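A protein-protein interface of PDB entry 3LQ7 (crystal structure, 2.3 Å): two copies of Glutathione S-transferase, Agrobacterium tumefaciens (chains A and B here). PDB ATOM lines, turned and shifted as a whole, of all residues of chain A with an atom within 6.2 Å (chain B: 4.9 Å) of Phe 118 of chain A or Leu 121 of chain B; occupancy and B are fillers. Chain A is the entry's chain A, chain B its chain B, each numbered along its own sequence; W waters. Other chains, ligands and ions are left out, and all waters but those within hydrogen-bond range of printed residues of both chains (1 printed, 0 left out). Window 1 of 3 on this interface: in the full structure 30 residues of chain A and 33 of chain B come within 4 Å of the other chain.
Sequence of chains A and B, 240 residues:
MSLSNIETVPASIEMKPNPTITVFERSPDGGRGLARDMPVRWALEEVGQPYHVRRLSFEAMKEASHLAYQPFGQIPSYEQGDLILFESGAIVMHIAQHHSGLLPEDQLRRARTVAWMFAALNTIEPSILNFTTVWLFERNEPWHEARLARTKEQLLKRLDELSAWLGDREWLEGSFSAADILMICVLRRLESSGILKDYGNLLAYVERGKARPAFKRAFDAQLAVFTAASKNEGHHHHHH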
ATOM      1  N   THR A 113     -22.332  -2.253  28.158  1.00  0.00           N
ATOM      2  CA  THR A 113     -22.118  -0.853  28.499  1.00  0.00           C
ATOM      3  C   THR A 113     -21.054  -0.225  27.592  1.00  0.00           C
ATOM      4  O   THR A 113     -21.281   0.847  27.020  1.00  0.00           O
ATOM      5  CB  THR A 113     -21.710  -0.692  29.971  1.00  0.00           C
ATOM      6  OG1 THR A 113     -22.632  -1.414  30.802  1.00  0.00           O
ATOM      7  CG2 THR A 113     -21.709   0.780  30.367  1.00  0.00           C
ATOM      8  N   VAL A 114     -19.922  -0.917  27.456  1.00  0.00           N
ATOM      9  CA  VAL A 114     -18.827  -0.532  26.552  1.00  0.00           C
ATOM     10  C   VAL A 114     -19.327  -0.358  25.109  1.00  0.00           C
ATOM     11  O   VAL A 114     -18.903   0.574  24.412  1.00  0.00           O
ATOM     12  CB  VAL A 114     -17.630  -1.539  26.645  1.00  0.00           C
ATOM     13  CG1 VAL A 114     -16.556  -1.273  25.585  1.00  0.00           C
ATOM     14  CG2 VAL A 114     -17.000  -1.476  28.022  1.00  0.00           C
ATOM     15  N   ALA A 115     -20.249  -1.231  24.691  1.00  0.00           N
ATOM     16  CA  ALA A 115     -20.891  -1.143  23.377  1.00  0.00           C
ATOM     17  C   ALA A 115     -21.625   0.173  23.188  1.00  0.00           C
ATOM     18  O   ALA A 115     -21.499   0.806  22.140  1.00  0.00           O
ATOM     19  CB  ALA A 115     -21.830  -2.330  23.140  1.00  0.00           C
ATOM     20  N   TRP A 116     -22.361   0.589  24.216  1.00  0.00           N
ATOM     21  CA  TRP A 116     -23.063   1.867  24.192  1.00  0.00           C
ATOM     22  C   TRP A 116     -22.126   3.079  24.237  1.00  0.00           C
ATOM     23  O   TRP A 116     -22.426   4.115  23.630  1.00  0.00           O
ATOM     24  CB  TRP A 116     -24.159   1.921  25.263  1.00  0.00           C
ATOM     25  CG  TRP A 116     -25.418   1.194  24.851  1.00  0.00           C
ATOM     26  CD1 TRP A 116     -25.931   0.058  25.406  1.00  0.00           C
ATOM     27  CD2 TRP A 116     -26.310   1.553  23.781  1.00  0.00           C
ATOM     28  NE1 TRP A 116     -27.092  -0.306  24.759  1.00  0.00           N
ATOM     29  CE2 TRP A 116     -27.342   0.594  23.757  1.00  0.00           C
ATOM     30  CE3 TRP A 116     -26.339   2.596  22.847  1.00  0.00           C
ATOM     31  CZ2 TRP A 116     -28.382   0.638  22.823  1.00  0.00           C
ATOM     32  CZ3 TRP A 116     -27.386   2.647  21.929  1.00  0.00           C
ATOM     33  CH2 TRP A 116     -28.390   1.674  21.925  1.00  0.00           C
ATOM     34  N   MET A 117     -20.990   2.931  24.919  1.00  0.00           N
ATOM     35  CA  MET A 117     -19.968   3.968  24.980  1.00  0.00           C
ATOM     36  C   MET A 117     -19.388   4.213  23.586  1.00  0.00           C
ATOM     37  O   MET A 117     -19.278   5.360  23.151  1.00  0.00           O
ATOM     38  CB  MET A 117     -18.849   3.596  25.966  1.00  0.00           C
ATOM     39  CG  MET A 117     -19.278   3.507  27.433  1.00  0.00           C
ATOM     40  SD  MET A 117     -17.962   2.985  28.563  1.00  0.00           S
ATOM     41  CE  MET A 117     -17.061   4.489  28.771  1.00  0.00           C
ATOM     42  N   PHE A 118     -19.027   3.132  22.895  1.00  0.00           N
ATOM     43  CA  PHE A 118     -18.577   3.211  21.508  1.00  0.00           C
ATOM     44  C   PHE A 118     -19.672   3.722  20.550  1.00  0.00           C
ATOM     45  O   PHE A 118     -19.377   4.535  19.680  1.00  0.00           O
ATOM     46  CB  PHE A 118     -18.021   1.861  21.028  1.00  0.00           C
ATOM     47  CG  PHE A 118     -16.572   1.637  21.378  1.00  0.00           C
ATOM     48  CD1 PHE A 118     -16.218   0.907  22.520  1.00  0.00           C
ATOM     49  CD2 PHE A 118     -15.559   2.156  20.572  1.00  0.00           C
ATOM     50  CE1 PHE A 118     -14.880   0.696  22.855  1.00  0.00           C
ATOM     51  CE2 PHE A 118     -14.212   1.950  20.892  1.00  0.00           C
ATOM     52  CZ  PHE A 118     -13.871   1.214  22.040  1.00  0.00           C
ATOM     53  N   ALA A 119     -20.913   3.254  20.733  1.00  0.00           N
ATOM     54  CA  ALA A 119     -22.066   3.665  19.922  1.00  0.00           C
ATOM     55  C   ALA A 119     -22.343   5.161  20.009  1.00  0.00           C
ATOM     56  O   ALA A 119     -22.612   5.798  18.996  1.00  0.00           O
ATOM     57  CB  ALA A 119     -23.315   2.887  20.310  1.00  0.00           C
ATOM     58  N   ALA A 120     -22.259   5.706  21.221  1.00  0.00           N
ATOM     59  CA  ALA A 120     -22.407   7.139  21.461  1.00  0.00           C
ATOM     60  C   ALA A 120     -21.475   7.993  20.606  1.00  0.00           C
ATOM     61  O   ALA A 120     -21.910   8.964  19.986  1.00  0.00           O
ATOM     62  CB  ALA A 120     -22.193   7.454  22.932  1.00  0.00           C
ATOM     63  N   LEU A 121     -20.209   7.592  20.559  1.00  0.00           N
ATOM     64  CA  LEU A 121     -19.149   8.407  19.994  1.00  0.00           C
ATOM     65  C   LEU A 121     -18.818   8.126  18.523  1.00  0.00           C
ATOM     66  O   LEU A 121     -18.401   9.037  17.806  1.00  0.00           O
ATOM     67  CB  LEU A 121     -17.888   8.294  20.858  1.00  0.00           C
ATOM     68  CG  LEU A 121     -18.003   8.847  22.288  1.00  0.00           C
ATOM     69  CD1 LEU A 121     -16.793   8.466  23.104  1.00  0.00           C
ATOM     70  CD2 LEU A 121     -18.187  10.365  22.314  1.00  0.00           C
ATOM     71  N   ASN A 122     -18.983   6.883  18.073  1.00  0.00           N
ATOM     72  CA  ASN A 122     -18.688   6.576  16.670  1.00  0.00           C
ATOM     73  C   ASN A 122     -19.900   6.349  15.763  1.00  0.00           C
ATOM     74  O   ASN A 122     -19.742   6.238  14.552  1.00  0.00           O
ATOM     75  CB  ASN A 122     -17.598   5.485  16.508  1.00  0.00           C
ATOM     76  CG  ASN A 122     -18.040   4.096  16.976  1.00  0.00           C
ATOM     77  OD1 ASN A 122     -17.267   3.383  17.617  1.00  0.00           O
ATOM     78  ND2 ASN A 122     -19.268   3.704  16.650  1.00  0.00           N
ATOM     79  N   THR A 123     -21.095   6.284  16.352  1.00  0.00           N
ATOM     80  CA  THR A 123     -22.325   6.079  15.587  1.00  0.00           C
ATOM     81  C   THR A 123     -23.299   7.265  15.691  1.00  0.00           C
ATOM     82  O   THR A 123     -23.784   7.765  14.669  1.00  0.00           O
ATOM     83  CB  THR A 123     -23.020   4.742  15.955  1.00  0.00           C
ATOM     84  OG1 THR A 123     -22.132   3.657  15.660  1.00  0.00           O
ATOM     85  CG2 THR A 123     -24.319   4.548  15.167  1.00  0.00           C
ATOM     86  N   ILE A 124     -23.571   7.727  16.908  1.00  0.00           N
ATOM     87  CA  ILE A 124     -24.535   8.815  17.086  1.00  0.00           C
ATOM     88  C   ILE A 124     -23.889  10.181  16.860  1.00  0.00           C
ATOM     89  O   ILE A 124     -24.420  11.008  16.106  1.00  0.00           O
ATOM     90  CB  ILE A 124     -25.304   8.728  18.437  1.00  0.00           C
ATOM     91  CG1 ILE A 124     -26.371   7.636  18.365  1.00  0.00           C
ATOM     92  CG2 ILE A 124     -26.073  10.007  18.729  1.00  0.00           C
ATOM     93  CD1 ILE A 124     -25.906   6.292  18.750  1.00  0.00           C
ATOM     94  N   PRO A 126     -21.109  11.327  15.081  1.00  0.00           N
ATOM     95  CA  PRO A 126     -20.813  11.846  13.732  1.00  0.00           C
ATOM     96  C   PRO A 126     -22.046  12.299  12.938  1.00  0.00           C
ATOM     97  O   PRO A 126     -21.960  13.284  12.203  1.00  0.00           O
ATOM     98  CB  PRO A 126     -20.125  10.663  13.035  1.00  0.00           C
ATOM     99  CG  PRO A 126     -19.523   9.878  14.159  1.00  0.00           C
ATOM    100  CD  PRO A 126     -20.538   9.973  15.262  1.00  0.00           C
ATOM    101  N   LEU A 182     -21.870   9.670  28.170  1.00  0.00           N
ATOM    102  CA  LEU A 182     -21.396   9.906  26.826  1.00  0.00           C
ATOM    103  C   LEU A 182     -22.554  10.178  25.864  1.00  0.00           C
ATOM    104  O   LEU A 182     -22.497  11.134  25.101  1.00  0.00           O
ATOM    105  CB  LEU A 182     -20.515   8.760  26.339  1.00  0.00           C
ATOM    106  CG  LEU A 182     -19.139   8.606  26.979  1.00  0.00           C
ATOM    107  CD1 LEU A 182     -18.403   7.447  26.322  1.00  0.00           C
ATOM    108  CD2 LEU A 182     -18.315   9.868  26.889  1.00  0.00           C
ATOM    109  N   GLU B  87     -21.161  -2.859  17.827  1.00  0.00           N
ATOM    110  CA  GLU B  87     -20.014  -1.940  17.744  1.00  0.00           C
ATOM    111  C   GLU B  87     -18.681  -2.665  17.677  1.00  0.00           C
ATOM    112  O   GLU B  87     -18.251  -3.284  18.660  1.00  0.00           O
ATOM    113  CB  GLU B  87     -20.008  -0.880  18.866  1.00  0.00           C
ATOM    114  CG  GLU B  87     -21.191   0.069  18.845  1.00  0.00           C
ATOM    115  CD  GLU B  87     -21.198   0.974  17.617  1.00  0.00           C
ATOM    116  OE1 GLU B  87     -22.285   1.454  17.239  1.00  0.00           O
ATOM    117  OE2 GLU B  87     -20.120   1.204  17.034  1.00  0.00           O
ATOM    118  N   GLY B  89     -15.676  -1.645  17.823  1.00  0.00           N
ATOM    119  CA  GLY B  89     -14.798  -1.262  18.923  1.00  0.00           C
ATOM    120  C   GLY B  89     -15.054  -2.040  20.203  1.00  0.00           C
ATOM    121  O   GLY B  89     -14.116  -2.437  20.884  1.00  0.00           O
ATOM    122  N   ALA B  90     -16.327  -2.256  20.520  1.00  0.00           N
ATOM    123  CA  ALA B  90     -16.733  -2.953  21.740  1.00  0.00           C
ATOM    124  C   ALA B  90     -16.501  -4.456  21.658  1.00  0.00           C
ATOM    125  O   ALA B  90     -16.096  -5.091  22.642  1.00  0.00           O
ATOM    126  CB  ALA B  90     -18.168  -2.684  22.022  1.00  0.00           C
ATOM    127  N   MET B  93     -12.841  -4.952  21.825  1.00  0.00           N
ATOM    128  CA  MET B  93     -12.454  -4.735  23.224  1.00  0.00           C
ATOM    129  C   MET B  93     -12.625  -6.001  24.047  1.00  0.00           C
ATOM    130  O   MET B  93     -11.681  -6.437  24.704  1.00  0.00           O
ATOM    131  CB  MET B  93     -13.234  -3.584  23.884  1.00  0.00           C
ATOM    132  CG  MET B  93     -12.443  -2.297  24.100  1.00  0.00           C
ATOM    133  SD  MET B  93     -11.321  -2.260  25.519  1.00  0.00           S
ATOM    134  CE  MET B  93      -9.834  -2.907  24.892  1.00  0.00           C
ATOM    135  N   MET B 117      -7.800   3.153  20.505  1.00  0.00           N
ATOM    136  CA  MET B 117      -8.972   2.444  19.976  1.00  0.00           C
ATOM    137  C   MET B 117     -10.122   3.427  19.762  1.00  0.00           C
ATOM    138  O   MET B 117     -10.863   3.330  18.782  1.00  0.00           O
ATOM    139  CB  MET B 117      -9.424   1.312  20.923  1.00  0.00           C
ATOM    140  CG  MET B 117      -8.377   0.214  21.219  1.00  0.00           C
ATOM    141  SD  MET B 117      -8.921  -1.060  22.408  1.00  0.00           S
ATOM    142  CE  MET B 117     -10.207  -1.783  21.400  1.00  0.00           C
ATOM    143  N   PHE B 118     -10.258   4.374  20.692  1.00  0.00           N
ATOM    144  CA  PHE B 118     -11.241   5.438  20.581  1.00  0.00           C
ATOM    145  C   PHE B 118     -10.882   6.458  19.485  1.00  0.00           C
ATOM    146  O   PHE B 118     -11.723   6.782  18.662  1.00  0.00           O
ATOM    147  CB  PHE B 118     -11.464   6.116  21.938  1.00  0.00           C
ATOM    148  CG  PHE B 118     -12.552   5.475  22.754  1.00  0.00           C
ATOM    149  CD1 PHE B 118     -12.240   4.562  23.763  1.00  0.00           C
ATOM    150  CD2 PHE B 118     -13.891   5.755  22.490  1.00  0.00           C
ATOM    151  CE1 PHE B 118     -13.249   3.957  24.514  1.00  0.00           C
ATOM    152  CE2 PHE B 118     -14.915   5.162  23.236  1.00  0.00           C
ATOM    153  CZ  PHE B 118     -14.592   4.256  24.252  1.00  0.00           C
ATOM    154  N   ALA B 119      -9.633   6.927  19.475  1.00  0.00           N
ATOM    155  CA  ALA B 119      -9.112   7.828  18.436  1.00  0.00           C
ATOM    156  C   ALA B 119      -9.271   7.292  17.012  1.00  0.00           C
ATOM    157  O   ALA B 119      -9.579   8.052  16.094  1.00  0.00           O
ATOM    158  CB  ALA B 119      -7.652   8.164  18.710  1.00  0.00           C
ATOM    159  N   ALA B 120      -9.078   5.986  16.835  1.00  0.00           N
ATOM    160  CA  ALA B 120      -9.226   5.351  15.527  1.00  0.00           C
ATOM    161  C   ALA B 120     -10.624   5.506  14.967  1.00  0.00           C
ATOM    162  O   ALA B 120     -10.781   5.835  13.794  1.00  0.00           O
ATOM    163  CB  ALA B 120      -8.851   3.872  15.596  1.00  0.00           C
ATOM    164  N   LEU B 121     -11.626   5.295  15.821  1.00  0.00           N
ATOM    165  CA  LEU B 121     -13.018   5.205  15.385  1.00  0.00           C
ATOM    166  C   LEU B 121     -13.829   6.496  15.499  1.00  0.00           C
ATOM    167  O   LEU B 121     -14.853   6.631  14.827  1.00  0.00           O
ATOM    168  CB  LEU B 121     -13.748   4.073  16.124  1.00  0.00           C
ATOM    169  CG  LEU B 121     -13.138   2.667  16.108  1.00  0.00           C
ATOM    170  CD1 LEU B 121     -13.966   1.750  16.973  1.00  0.00           C
ATOM    171  CD2 LEU B 121     -12.998   2.095  14.704  1.00  0.00           C
ATOM    172  N   ASN B 122     -13.394   7.435  16.340  1.00  0.00           N
ATOM    173  CA  ASN B 122     -14.114   8.712  16.447  1.00  0.00           C
ATOM    174  C   ASN B 122     -13.362   9.992  16.060  1.00  0.00           C
ATOM    175  O   ASN B 122     -13.979  11.054  15.954  1.00  0.00           O
ATOM    176  CB  ASN B 122     -14.865   8.855  17.790  1.00  0.00           C
ATOM    177  CG  ASN B 122     -13.948   8.915  19.010  1.00  0.00           C
ATOM    178  OD1 ASN B 122     -14.388   8.631  20.123  1.00  0.00           O
ATOM    179  ND2 ASN B 122     -12.688   9.287  18.817  1.00  0.00           N
ATOM    180  N   THR B 123     -12.049   9.881  15.849  1.00  0.00           N
ATOM    181  CA  THR B 123     -11.215  11.013  15.432  1.00  0.00           C
ATOM    182  C   THR B 123     -10.707  10.828  14.000  1.00  0.00           C
ATOM    183  O   THR B 123     -10.824  11.736  13.186  1.00  0.00           O
ATOM    184  CB  THR B 123     -10.015  11.236  16.392  1.00  0.00           C
ATOM    185  OG1 THR B 123     -10.491  11.405  17.730  1.00  0.00           O
ATOM    186  CG2 THR B 123      -9.204  12.470  15.998  1.00  0.00           C
ATOM    187  N   GLU B 125     -11.435   7.911  11.769  1.00  0.00           N
ATOM    188  CA  GLU B 125     -12.450   7.305  10.897  1.00  0.00           C
ATOM    189  C   GLU B 125     -13.565   8.232  10.357  1.00  0.00           C
ATOM    190  O   GLU B 125     -13.976   8.050   9.211  1.00  0.00           O
ATOM    191  CB  GLU B 125     -13.065   6.078  11.570  1.00  0.00           C
ATOM    192  CG  GLU B 125     -13.940   5.205  10.685  1.00  0.00           C
ATOM    193  CD  GLU B 125     -14.870   4.332  11.494  1.00  0.00           C
ATOM    194  OE1 GLU B 125     -15.640   4.881  12.315  1.00  0.00           O
ATOM    195  OE2 GLU B 125     -14.832   3.098  11.311  1.00  0.00           O
ATOM    196  N   PRO B 126     -14.075   9.199  11.166  1.00  0.00           N
ATOM    197  CA  PRO B 126     -15.103  10.054  10.554  1.00  0.00           C
ATOM    198  C   PRO B 126     -14.563  10.956   9.434  1.00  0.00           C
ATOM    199  O   PRO B 126     -15.234  11.113   8.417  1.00  0.00           O
ATOM    200  CB  PRO B 126     -15.636  10.878  11.736  1.00  0.00           C
ATOM    201  CG  PRO B 126     -15.296  10.081  12.945  1.00  0.00           C
ATOM    202  CD  PRO B 126     -13.976   9.452  12.619  1.00  0.00           C
ATOM    203  N   LEU B 182      -7.742  -1.836  14.856  1.00  0.00           N
ATOM    204  CA  LEU B 182      -8.778  -0.870  14.535  1.00  0.00           C
ATOM    205  C   LEU B 182      -8.269   0.238  13.601  1.00  0.00           C
ATOM    206  O   LEU B 182      -8.931   0.547  12.620  1.00  0.00           O
ATOM    207  CB  LEU B 182      -9.438  -0.320  15.798  1.00  0.00           C
ATOM    208  CG  LEU B 182     -10.337  -1.313  16.552  1.00  0.00           C
ATOM    209  CD1 LEU B 182     -10.931  -0.661  17.793  1.00  0.00           C
ATOM    210  CD2 LEU B 182     -11.447  -1.847  15.666  1.00  0.00           C
ATOM    211  N   VAL B 186      -9.256   0.908   9.654  1.00  0.00           N
ATOM    212  CA  VAL B 186      -9.764   2.245   9.352  1.00  0.00           C
ATOM    213  C   VAL B 186      -8.985   2.874   8.177  1.00  0.00           C
ATOM    214  O   VAL B 186      -9.587   3.346   7.212  1.00  0.00           O
ATOM    215  CB  VAL B 186      -9.774   3.140  10.627  1.00  0.00           C
ATOM    216  CG1 VAL B 186      -9.741   4.600  10.288  1.00  0.00           C
ATOM    217  CG2 VAL B 186     -10.999   2.839  11.476  1.00  0.00           C
HETATM  218  O   HOH W   1     -17.379   0.595  17.201  1.00  0.00           O
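Hydrophobic or aromatic side chains of chain A within 4 Å of the printed part of chain B: Ala 115, Phe 118, Ala 119 and Leu 121. Of the 15 printed residues of chain B, 6 touch a printed residue of chain A. Hydrophobic or aromatic side chains of chain B that line the printed part of chain A: Ala 90, Phe 118 and Leu 121. Among the printed residues, 12 pairs touch across the chains.
Phe 118 of chain B touches its own counterpart, Phe 118 of chain A. Phe 118 of chain A touches Leu 121 of chain B, and with the chains exchanged Leu 121 of chain A touches Phe 118 of chain B. Leu 121 of chain A touches Asn 122 of chain B, and with the chains exchanged Asn 122 of chain A touches Leu 121 of chain B. Positions printed for both chains: 117, 118, 119, 120, 121, 122, 123, 126 and 182. Of the 12 pairs that touch across the chains among the printed residues, 5 have their exchanged pair printed and touching as well.
The side-chain carboxylate of Glu 87 of chain B lies within hydrogen-bond range of the side-chain amide nitrogen of Asn 122 of chain A, at 2.7 Å. The side-chain hydroxyl of Thr 123 of chain A lies within hydrogen-bond range of the side-chain carboxylate of Glu 87 of chain B, 2.7 Å away.
Ala 115 of chain A touches Glu 87 of chain B. CA of Ala 115 of chain A touches CB of Ala 90 of chain B, at 3.4 Å. CE1 of Phe 118 of chain A touches O of Gly 89 of chain B, 3.8 Å away. Phe 118 of chain A touches Ala 90 of chain B. CE1 of Phe 118 of chain B touches CZ of Phe 118 of chain A, 3.7 Å away. Phe 118 of chain A touches Leu 121 of chain B. Glu 87 of chain B touches Ala 119 of chain A. Phe 118 of chain B touches Leu 121 of chain A (CE2 to CD1, 3.8 Å). Asn 122 of chain B touches Leu 121 of chain A. Asn 122 of chain A touches Leu 121 of chain B (CB to O, 3.4 Å).
O of Phe 118 of chain A lies close to ND2 of Asn 122 of chain A. The backbone carbonyl oxygen of Ala 119 of chain A lies within hydrogen-bond range of the backbone NH of Ile 124 of chain A (3.0 Å). The side-chain hydroxyl (OG1) of Thr 123 of chain A sits at hydrogen-bond distance from the side-chain amide nitrogen (ND2) of Asn 122 of chain A (3.0 Å). O of Phe 118 of chain B is in hydrogen-bond range of ND2 of Asn 122 of chain B (2.7 Å). The side-chain hydroxyl (OG1) of Thr 123 of chain B lies within hydrogen-bond range of the side-chain amide nitrogen (ND2) of Asn 122 of chain B (3.2 Å).
Water W1 lies within hydrogen-bond range of the side-chain carboxylate of Glu 87 of chain B (2.8 Å), the side-chain amide oxygen of Asn 122 of chain A (2.8 Å) and the backbone NH of Gly 89 of chain B (2.9 Å).
Val 114 of chain A touches none of the printed residues of chain B. Printed residues of chain B within 4 Å of Phe 118 of chain A: Gly 89 (3.8 Å), Ala 90 (3.7 Å), Phe 118 (3.7 Å) and Leu 121 (3.9 Å). Of the printed residues of chain B, Ala 119 of chain A touches Glu 87. Printed residues of chain B within 4 Å of Leu 121 of chain A: Phe 118 (3.8 Å) and Asn 122 (3.5 Å). Ile 124 of chain A touches none of the printed residues of chain B. Of the printed residues of chain A, Gly 89 of chain B touches Phe 118. Printed residues of chain A within 4 Å of Phe 118 of chain B: Phe 118 and Leu 121. Leu 121 of chain B touches two residues of chain A. Of the printed residues of chain A, Asn 122 of chain B touches Leu 121. The nearest printed residue of chain B that does not touch Phe 118 of chain A is Glu 87 of chain B (4.02 Å). The nearest residue of chain A that does not touch Leu 121 of chain B is Leu 121 of chain A (5.2 Å).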
